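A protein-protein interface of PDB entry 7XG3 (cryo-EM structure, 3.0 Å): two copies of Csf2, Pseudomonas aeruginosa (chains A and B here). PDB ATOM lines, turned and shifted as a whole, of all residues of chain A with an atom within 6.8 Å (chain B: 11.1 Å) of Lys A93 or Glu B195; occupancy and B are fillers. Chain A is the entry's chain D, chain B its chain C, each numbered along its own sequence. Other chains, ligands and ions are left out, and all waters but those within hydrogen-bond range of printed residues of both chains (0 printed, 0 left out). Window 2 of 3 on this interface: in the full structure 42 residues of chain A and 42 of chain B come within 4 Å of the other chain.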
ATOM      1  N   GLU A  84      10.358   1.426   2.962  1.00  0.00           N
ATOM      2  CA  GLU A  84      11.502   0.827   3.648  1.00  0.00           C
ATOM      3  C   GLU A  84      11.458   0.875   5.182  1.00  0.00           C
ATOM      4  O   GLU A  84      12.084   0.003   5.792  1.00  0.00           O
ATOM      5  CB  GLU A  84      12.846   1.379   3.130  1.00  0.00           C
ATOM      6  CG  GLU A  84      12.978   2.855   2.838  1.00  0.00           C
ATOM      7  CD  GLU A  84      14.386   3.255   2.440  1.00  0.00           C
ATOM      8  OE1 GLU A  84      14.981   4.100   3.143  1.00  0.00           O
ATOM      9  OE2 GLU A  84      14.895   2.731   1.426  1.00  0.00           O
ATOM     10  N   PRO A  85      10.785   1.857   5.881  1.00  0.00           N
ATOM     11  CA  PRO A  85      10.548   1.651   7.323  1.00  0.00           C
ATOM     12  C   PRO A  85       9.761   0.397   7.682  1.00  0.00           C
ATOM     13  O   PRO A  85      10.160  -0.340   8.589  1.00  0.00           O
ATOM     14  CB  PRO A  85       9.768   2.902   7.740  1.00  0.00           C
ATOM     15  CG  PRO A  85      10.168   3.927   6.812  1.00  0.00           C
ATOM     16  CD  PRO A  85      10.670   3.293   5.553  1.00  0.00           C
ATOM     17  N   LEU A  87       9.557  -2.122   5.795  1.00  0.00           N
ATOM     18  CA  LEU A  87      10.274  -3.213   5.158  1.00  0.00           C
ATOM     19  C   LEU A  87      11.544  -3.611   5.902  1.00  0.00           C
ATOM     20  O   LEU A  87      12.020  -4.738   5.724  1.00  0.00           O
ATOM     21  CB  LEU A  87      10.595  -2.815   3.719  1.00  0.00           C
ATOM     22  CG  LEU A  87      10.961  -3.854   2.673  1.00  0.00           C
ATOM     23  CD1 LEU A  87       9.723  -4.454   2.063  1.00  0.00           C
ATOM     24  CD2 LEU A  87      11.731  -3.126   1.623  1.00  0.00           C
ATOM     25  N   VAL A  88      12.105  -2.723   6.731  1.00  0.00           N
ATOM     26  CA  VAL A  88      13.145  -3.108   7.681  1.00  0.00           C
ATOM     27  C   VAL A  88      12.578  -3.434   9.048  1.00  0.00           C
ATOM     28  O   VAL A  88      13.339  -3.796   9.955  1.00  0.00           O
ATOM     29  CB  VAL A  88      14.236  -2.027   7.832  1.00  0.00           C
ATOM     30  CG1 VAL A  88      14.843  -1.680   6.489  1.00  0.00           C
ATOM     31  CG2 VAL A  88      13.687  -0.795   8.547  1.00  0.00           C
ATOM     32  N   LYS A  90      10.749  -5.994   9.473  1.00  0.00           N
ATOM     33  CA  LYS A  90      11.135  -7.392   9.427  1.00  0.00           C
ATOM     34  C   LYS A  90      12.432  -7.501   8.635  1.00  0.00           C
ATOM     35  O   LYS A  90      13.032  -6.496   8.245  1.00  0.00           O
ATOM     36  CB  LYS A  90      10.030  -8.261   8.813  1.00  0.00           C
ATOM     37  CG  LYS A  90       8.649  -7.990   9.402  1.00  0.00           C
ATOM     38  CD  LYS A  90       7.532  -8.693   8.634  1.00  0.00           C
ATOM     39  CE  LYS A  90       7.672  -8.541   7.127  1.00  0.00           C
ATOM     40  NZ  LYS A  90       6.529  -9.156   6.400  1.00  0.00           N
ATOM     41  N   GLY A  91      12.864  -8.732   8.389  1.00  0.00           N
ATOM     42  CA  GLY A  91      14.166  -8.960   7.791  1.00  0.00           C
ATOM     43  C   GLY A  91      14.246  -8.848   6.280  1.00  0.00           C
ATOM     44  O   GLY A  91      15.137  -9.442   5.666  1.00  0.00           O
ATOM     45  N   ASN A  92      13.337  -8.099   5.664  1.00  0.00           N
ATOM     46  CA  ASN A  92      13.365  -7.945   4.217  1.00  0.00           C
ATOM     47  C   ASN A  92      14.426  -6.935   3.803  1.00  0.00           C
ATOM     48  O   ASN A  92      14.503  -5.830   4.345  1.00  0.00           O
ATOM     49  CB  ASN A  92      11.994  -7.512   3.703  1.00  0.00           C
ATOM     50  CG  ASN A  92      10.862  -8.248   4.386  1.00  0.00           C
ATOM     51  OD1 ASN A  92      10.524  -7.960   5.533  1.00  0.00           O
ATOM     52  ND2 ASN A  92      10.272  -9.209   3.685  1.00  0.00           N
ATOM     53  N   LYS A  93      15.248  -7.323   2.832  1.00  0.00           N
ATOM     54  CA  LYS A  93      16.309  -6.459   2.339  1.00  0.00           C
ATOM     55  C   LYS A  93      16.365  -6.555   0.823  1.00  0.00           C
ATOM     56  O   LYS A  93      15.960  -7.555   0.225  1.00  0.00           O
ATOM     57  CB  LYS A  93      17.669  -6.827   2.944  1.00  0.00           C
ATOM     58  CG  LYS A  93      17.891  -6.328   4.362  1.00  0.00           C
ATOM     59  CD  LYS A  93      19.367  -6.365   4.726  1.00  0.00           C
ATOM     60  CE  LYS A  93      19.570  -6.290   6.229  1.00  0.00           C
ATOM     61  NZ  LYS A  93      19.061  -5.019   6.806  1.00  0.00           N
ATOM     62  N   LEU A  94      16.885  -5.500   0.207  1.00  0.00           N
ATOM     63  CA  LEU A  94      17.028  -5.408  -1.237  1.00  0.00           C
ATOM     64  C   LEU A  94      18.493  -5.476  -1.626  1.00  0.00           C
ATOM     65  O   LEU A  94      19.375  -5.147  -0.833  1.00  0.00           O
ATOM     66  CB  LEU A  94      16.424  -4.108  -1.786  1.00  0.00           C
ATOM     67  CG  LEU A  94      14.943  -4.055  -2.158  1.00  0.00           C
ATOM     68  CD1 LEU A  94      14.071  -4.156  -0.956  1.00  0.00           C
ATOM     69  CD2 LEU A  94      14.656  -2.749  -2.874  1.00  0.00           C
ATOM     70  N   SER A  95      18.746  -5.901  -2.858  1.00  0.00           N
ATOM     71  CA  SER A  95      20.067  -5.695  -3.419  1.00  0.00           C
ATOM     72  C   SER A  95      20.246  -4.221  -3.769  1.00  0.00           C
ATOM     73  O   SER A  95      19.293  -3.434  -3.785  1.00  0.00           O
ATOM     74  CB  SER A  95      20.287  -6.569  -4.653  1.00  0.00           C
ATOM     75  OG  SER A  95      19.132  -6.612  -5.469  1.00  0.00           O
ATOM     76  N   ALA A  98      18.424  -3.426  -6.711  1.00  0.00           N
ATOM     77  CA  ALA A  98      17.003  -3.312  -6.401  1.00  0.00           C
ATOM     78  C   ALA A  98      16.693  -1.977  -5.735  1.00  0.00           C
ATOM     79  O   ALA A  98      15.629  -1.394  -5.966  1.00  0.00           O
ATOM     80  CB  ALA A  98      16.564  -4.482  -5.525  1.00  0.00           C
ATOM     81  N   SER A 335      10.325  -8.006  -0.123  1.00  0.00           N
ATOM     82  CA  SER A 335      11.317  -7.496  -1.058  1.00  0.00           C
ATOM     83  C   SER A 335      11.317  -8.230  -2.390  1.00  0.00           C
ATOM     84  O   SER A 335      11.846  -7.687  -3.372  1.00  0.00           O
ATOM     85  CB  SER A 335      12.709  -7.579  -0.436  1.00  0.00           C
ATOM     86  OG  SER A 335      13.216  -8.899  -0.497  1.00  0.00           O
ATOM     87  N   LYS A 336      10.718  -9.428  -2.443  1.00  0.00           N
ATOM     88  CA  LYS A 336      10.870 -10.313  -3.597  1.00  0.00           C
ATOM     89  C   LYS A 336      10.264  -9.707  -4.855  1.00  0.00           C
ATOM     90  O   LYS A 336      10.751  -9.954  -5.963  1.00  0.00           O
ATOM     91  CB  LYS A 336      10.240 -11.675  -3.305  1.00  0.00           C
ATOM     92  CG  LYS A 336       8.837 -11.602  -2.723  1.00  0.00           C
ATOM     93  CD  LYS A 336       8.267 -12.987  -2.471  1.00  0.00           C
ATOM     94  CE  LYS A 336       6.774 -12.923  -2.189  1.00  0.00           C
ATOM     95  NZ  LYS A 336       6.459 -12.239  -0.904  1.00  0.00           N
ATOM     96  N   GLU A 339      13.047  -7.506  -6.104  1.00  0.00           N
ATOM     97  CA  GLU A 339      14.064  -8.279  -6.819  1.00  0.00           C
ATOM     98  C   GLU A 339      13.573  -8.722  -8.194  1.00  0.00           C
ATOM     99  O   GLU A 339      14.254  -8.490  -9.198  1.00  0.00           O
ATOM    100  CB  GLU A 339      14.574  -9.509  -6.050  1.00  0.00           C
ATOM    101  CG  GLU A 339      15.613  -9.253  -4.950  1.00  0.00           C
ATOM    102  CD  GLU A 339      15.064  -8.705  -3.666  1.00  0.00           C
ATOM    103  OE1 GLU A 339      14.096  -9.302  -3.162  1.00  0.00           O
ATOM    104  OE2 GLU A 339      15.567  -7.675  -3.171  1.00  0.00           O
ATOM    105  N   ILE B 185      22.561   5.789  -5.117  1.00  0.00           N
ATOM    106  CA  ILE B 185      23.494   5.296  -4.111  1.00  0.00           C
ATOM    107  C   ILE B 185      24.308   6.452  -3.544  1.00  0.00           C
ATOM    108  O   ILE B 185      24.631   6.482  -2.347  1.00  0.00           O
ATOM    109  CB  ILE B 185      24.360   4.177  -4.720  1.00  0.00           C
ATOM    110  CG1 ILE B 185      23.479   2.958  -4.953  1.00  0.00           C
ATOM    111  CG2 ILE B 185      25.511   3.771  -3.821  1.00  0.00           C
ATOM    112  CD1 ILE B 185      23.086   2.734  -6.356  1.00  0.00           C
ATOM    113  N   ASN B 187      23.047   9.291  -3.064  1.00  0.00           N
ATOM    114  CA  ASN B 187      22.082   9.980  -2.215  1.00  0.00           C
ATOM    115  C   ASN B 187      21.973   9.342  -0.823  1.00  0.00           C
ATOM    116  O   ASN B 187      21.359   9.929   0.077  1.00  0.00           O
ATOM    117  CB  ASN B 187      20.723  10.005  -2.937  1.00  0.00           C
ATOM    118  CG  ASN B 187      19.667  10.819  -2.209  1.00  0.00           C
ATOM    119  OD1 ASN B 187      18.532  10.376  -2.039  1.00  0.00           O
ATOM    120  ND2 ASN B 187      20.042  12.013  -1.764  1.00  0.00           N
ATOM    121  N   LEU B 188      22.600   8.183  -0.614  1.00  0.00           N
ATOM    122  CA  LEU B 188      22.476   7.455   0.645  1.00  0.00           C
ATOM    123  C   LEU B 188      23.170   8.196   1.782  1.00  0.00           C
ATOM    124  O   LEU B 188      24.372   8.473   1.721  1.00  0.00           O
ATOM    125  CB  LEU B 188      23.068   6.057   0.503  1.00  0.00           C
ATOM    126  CG  LEU B 188      22.153   4.966  -0.044  1.00  0.00           C
ATOM    127  CD1 LEU B 188      22.974   3.855  -0.673  1.00  0.00           C
ATOM    128  CD2 LEU B 188      21.290   4.426   1.073  1.00  0.00           C
ATOM    129  N   GLY B 189      22.405   8.506   2.826  1.00  0.00           N
ATOM    130  CA  GLY B 189      22.900   9.319   3.916  1.00  0.00           C
ATOM    131  C   GLY B 189      23.712   8.599   4.972  1.00  0.00           C
ATOM    132  O   GLY B 189      24.895   8.898   5.160  1.00  0.00           O
ATOM    133  N   SER B 190      23.100   7.642   5.659  1.00  0.00           N
ATOM    134  CA  SER B 190      23.703   7.061   6.851  1.00  0.00           C
ATOM    135  C   SER B 190      23.295   5.596   6.948  1.00  0.00           C
ATOM    136  O   SER B 190      22.829   4.994   5.978  1.00  0.00           O
ATOM    137  CB  SER B 190      23.296   7.840   8.104  1.00  0.00           C
ATOM    138  OG  SER B 190      21.937   8.232   8.036  1.00  0.00           O
ATOM    139  N   SER B 191      23.489   5.026   8.140  1.00  0.00           N
ATOM    140  CA  SER B 191      23.236   3.603   8.348  1.00  0.00           C
ATOM    141  C   SER B 191      21.748   3.283   8.330  1.00  0.00           C
ATOM    142  O   SER B 191      21.349   2.175   7.952  1.00  0.00           O
ATOM    143  CB  SER B 191      23.861   3.152   9.668  1.00  0.00           C
ATOM    144  OG  SER B 191      23.231   3.783  10.769  1.00  0.00           O
ATOM    145  N   GLU B 192      20.911   4.235   8.748  1.00  0.00           N
ATOM    146  CA  GLU B 192      19.469   4.008   8.741  1.00  0.00           C
ATOM    147  C   GLU B 192      18.916   3.994   7.321  1.00  0.00           C
ATOM    148  O   GLU B 192      17.943   3.288   7.034  1.00  0.00           O
ATOM    149  CB  GLU B 192      18.761   5.070   9.583  1.00  0.00           C
ATOM    150  CG  GLU B 192      19.246   6.492   9.346  1.00  0.00           C
ATOM    151  CD  GLU B 192      20.297   6.923  10.348  1.00  0.00           C
ATOM    152  OE1 GLU B 192      20.698   6.090  11.188  1.00  0.00           O
ATOM    153  OE2 GLU B 192      20.729   8.093  10.288  1.00  0.00           O
ATOM    154  N   ASP B 193      19.520   4.767   6.419  1.00  0.00           N
ATOM    155  CA  ASP B 193      19.069   4.774   5.033  1.00  0.00           C
ATOM    156  C   ASP B 193      19.616   3.589   4.248  1.00  0.00           C
ATOM    157  O   ASP B 193      19.042   3.217   3.220  1.00  0.00           O
ATOM    158  CB  ASP B 193      19.478   6.083   4.354  1.00  0.00           C
ATOM    159  CG  ASP B 193      18.659   7.269   4.831  1.00  0.00           C
ATOM    160  OD1 ASP B 193      18.056   7.179   5.920  1.00  0.00           O
ATOM    161  OD2 ASP B 193      18.621   8.293   4.116  1.00  0.00           O
ATOM    162  N   VAL B 194      20.705   2.979   4.719  1.00  0.00           N
ATOM    163  CA  VAL B 194      21.401   1.944   3.959  1.00  0.00           C
ATOM    164  C   VAL B 194      21.118   0.538   4.483  1.00  0.00           C
ATOM    165  O   VAL B 194      21.545  -0.445   3.853  1.00  0.00           O
ATOM    166  CB  VAL B 194      22.920   2.236   3.936  1.00  0.00           C
ATOM    167  CG1 VAL B 194      23.634   1.666   5.167  1.00  0.00           C
ATOM    168  CG2 VAL B 194      23.570   1.785   2.626  1.00  0.00           C
ATOM    169  N   GLU B 195      20.370   0.410   5.583  1.00  0.00           N
ATOM    170  CA  GLU B 195      20.159  -0.896   6.207  1.00  0.00           C
ATOM    171  C   GLU B 195      19.260  -1.797   5.365  1.00  0.00           C
ATOM    172  O   GLU B 195      19.291  -3.024   5.515  1.00  0.00           O
ATOM    173  CB  GLU B 195      19.572  -0.715   7.605  1.00  0.00           C
ATOM    174  CG  GLU B 195      18.245   0.018   7.631  1.00  0.00           C
ATOM    175  CD  GLU B 195      17.771   0.293   9.039  1.00  0.00           C
ATOM    176  OE1 GLU B 195      18.452  -0.143   9.990  1.00  0.00           O
ATOM    177  OE2 GLU B 195      16.716   0.942   9.200  1.00  0.00           O
ATOM    178  N   VAL B 196      18.458  -1.214   4.471  1.00  0.00           N
ATOM    179  CA  VAL B 196      17.610  -2.021   3.602  1.00  0.00           C
ATOM    180  C   VAL B 196      18.411  -2.667   2.474  1.00  0.00           C
ATOM    181  O   VAL B 196      17.925  -3.603   1.831  1.00  0.00           O
ATOM    182  CB  VAL B 196      16.442  -1.158   3.073  1.00  0.00           C
ATOM    183  CG1 VAL B 196      16.844  -0.388   1.836  1.00  0.00           C
ATOM    184  CG2 VAL B 196      15.205  -2.011   2.796  1.00  0.00           C
ATOM    185  N   ILE B 197      19.637  -2.208   2.222  1.00  0.00           N
ATOM    186  CA  ILE B 197      20.454  -2.799   1.170  1.00  0.00           C
ATOM    187  C   ILE B 197      21.147  -4.046   1.702  1.00  0.00           C
ATOM    188  O   ILE B 197      21.779  -4.017   2.766  1.00  0.00           O
ATOM    189  CB  ILE B 197      21.472  -1.779   0.642  1.00  0.00           C
ATOM    190  CG1 ILE B 197      20.768  -0.699  -0.176  1.00  0.00           C
ATOM    191  CG2 ILE B 197      22.539  -2.459  -0.202  1.00  0.00           C
ATOM    192  CD1 ILE B 197      20.690   0.630   0.523  1.00  0.00           C
ATOM    193  N   ASN B 198      21.013  -5.157   0.972  1.00  0.00           N
ATOM    194  CA  ASN B 198      21.830  -6.338   1.225  1.00  0.00           C
ATOM    195  C   ASN B 198      23.295  -6.001   0.970  1.00  0.00           C
ATOM    196  O   ASN B 198      23.677  -5.668  -0.157  1.00  0.00           O
ATOM    197  CB  ASN B 198      21.382  -7.495   0.338  1.00  0.00           C
ATOM    198  CG  ASN B 198      20.536  -8.503   1.081  1.00  0.00           C
ATOM    199  OD1 ASN B 198      20.473  -8.488   2.310  1.00  0.00           O
ATOM    200  ND2 ASN B 198      19.873  -9.381   0.340  1.00  0.00           N
ATOM    201  N   GLY B 199      24.112  -6.085   2.019  1.00  0.00           N
ATOM    202  CA  GLY B 199      25.461  -5.582   2.020  1.00  0.00           C
ATOM    203  C   GLY B 199      25.580  -4.199   2.627  1.00  0.00           C
ATOM    204  O   GLY B 199      26.521  -3.943   3.387  1.00  0.00           O
ATOM    205  N   GLY B 200      24.636  -3.313   2.316  1.00  0.00           N
ATOM    206  CA  GLY B 200      24.565  -2.016   2.964  1.00  0.00           C
ATOM    207  C   GLY B 200      25.702  -1.105   2.562  1.00  0.00           C
ATOM    208  O   GLY B 200      25.796  -0.652   1.411  1.00  0.00           O
ATOM    209  N   ALA B 201      26.572  -0.832   3.538  1.00  0.00           N
ATOM    210  CA  ALA B 201      27.714   0.044   3.313  1.00  0.00           C
ATOM    211  C   ALA B 201      28.691  -0.561   2.315  1.00  0.00           C
ATOM    212  O   ALA B 201      29.240   0.153   1.470  1.00  0.00           O
ATOM    213  CB  ALA B 201      28.413   0.342   4.638  1.00  0.00           C
ATOM    214  N   VAL B 202      28.893  -1.879   2.385  1.00  0.00           N
ATOM    215  CA  VAL B 202      29.827  -2.555   1.486  1.00  0.00           C
ATOM    216  C   VAL B 202      29.321  -2.511   0.049  1.00  0.00           C
ATOM    217  O   VAL B 202      30.080  -2.222  -0.882  1.00  0.00           O
ATOM    218  CB  VAL B 202      30.065  -4.001   1.957  1.00  0.00           C
ATOM    219  CG1 VAL B 202      31.149  -4.663   1.122  1.00  0.00           C
ATOM    220  CG2 VAL B 202      30.426  -4.023   3.432  1.00  0.00           C
ATOM    221  N   ALA B 203      28.022  -2.771  -0.148  1.00  0.00           N
ATOM    222  CA  ALA B 203      27.447  -2.753  -1.491  1.00  0.00           C
ATOM    223  C   ALA B 203      27.413  -1.342  -2.068  1.00  0.00           C
ATOM    224  O   ALA B 203      27.711  -1.141  -3.257  1.00  0.00           O
ATOM    225  CB  ALA B 203      26.042  -3.353  -1.463  1.00  0.00           C
ATOM    226  N   ALA B 204      27.061  -0.354  -1.236  1.00  0.00           N
ATOM    227  CA  ALA B 204      27.040   1.037  -1.681  1.00  0.00           C
ATOM    228  C   ALA B 204      28.437   1.520  -2.051  1.00  0.00           C
ATOM    229  O   ALA B 204      28.628   2.173  -3.088  1.00  0.00           O
ATOM    230  CB  ALA B 204      26.433   1.920  -0.591  1.00  0.00           C
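The backbone carbonyl oxygen (O) of Val B196 sits at hydrogen-bond distance from the backbone NH (N) of Leu A94 (2.7 Å). The backbone NH (N) of Asn B198 lies within hydrogen-bond range of the backbone carbonyl oxygen (O) of Leu A94 (2.4 Å). The side-chain amino group (NZ) of Lys A93 lies close to the backbone carbonyl oxygen (O) of Glu B195 (2.4 Å).
The side-chain hydroxyl (OG) of Ser A335 is in hydrogen-bond range of the backbone carbonyl oxygen (O) of Lys A93, at 3.1 Å.
Among the printed residues, pairs that only touch across the chains: Leu A94 with Ile B197 (3.3 Å), Lys A93 with Asn B198 (3.3 Å), Lys A93 with Val B196 (3.3 Å), Val A88 with Glu B195 (3.6 Å), Glu A84 with Val B196 (3.7 Å), Val A88 with Val B196 (3.7 Å), Leu A87 with Val B196 (3.8 Å) and Lys A93 with Ile B197 (3.9 Å).
Of the printed residues of chain B, Glu A84 touches Val B196. Val A88 touches just these residues of chain B: Glu B195 (3.6 Å) and Val B196 (3.7 Å). No residue of chain B comes within 4 Å of Gly A91. No residue of chain B comes within 4 Å of Asn A92. Lys A93 touches just these residues of chain B: Glu B195 (2.4 Å), Val B196 (3.3 Å), Ile B197 (3.9 Å) and Asn B198 (3.3 Å). Ser A95 touches none of the printed residues of chain B. Ser A335 touches none of the printed residues of chain B. Glu B192 touches none of the printed residues of chain A. Glu B195 touches just these residues of chain A: Val A88 (3.6 Å) and Lys A93 (2.4 Å). Of the printed residues of chain A, Ile B197 touches Lys A93 (3.9 Å) and Leu A94 (3.3 Å). Ala B204 touches none of the printed residues of chain A.
Of the 14 printed residues of chain A, 5 touch a printed residue of chain B. Printed residues of chain A that touch a printed residue of chain B: Glu A84, Leu A87, Val A88, Lys A93 and Leu A94. Hydrophobic or aromatic side chains of chain B that line the printed part of chain A: Val B196. Among the printed residues, 11 pairs touch across the chains. Among the printed residues, no Asp or Glu carboxylate lies within 4 Å of a Lys or Arg side-chain nitrogen of the other chain.
No position is printed for both chains. Of the 11 pairs that touch across the chains among the printed residues, none has its exchanged pair printed and touching as well.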
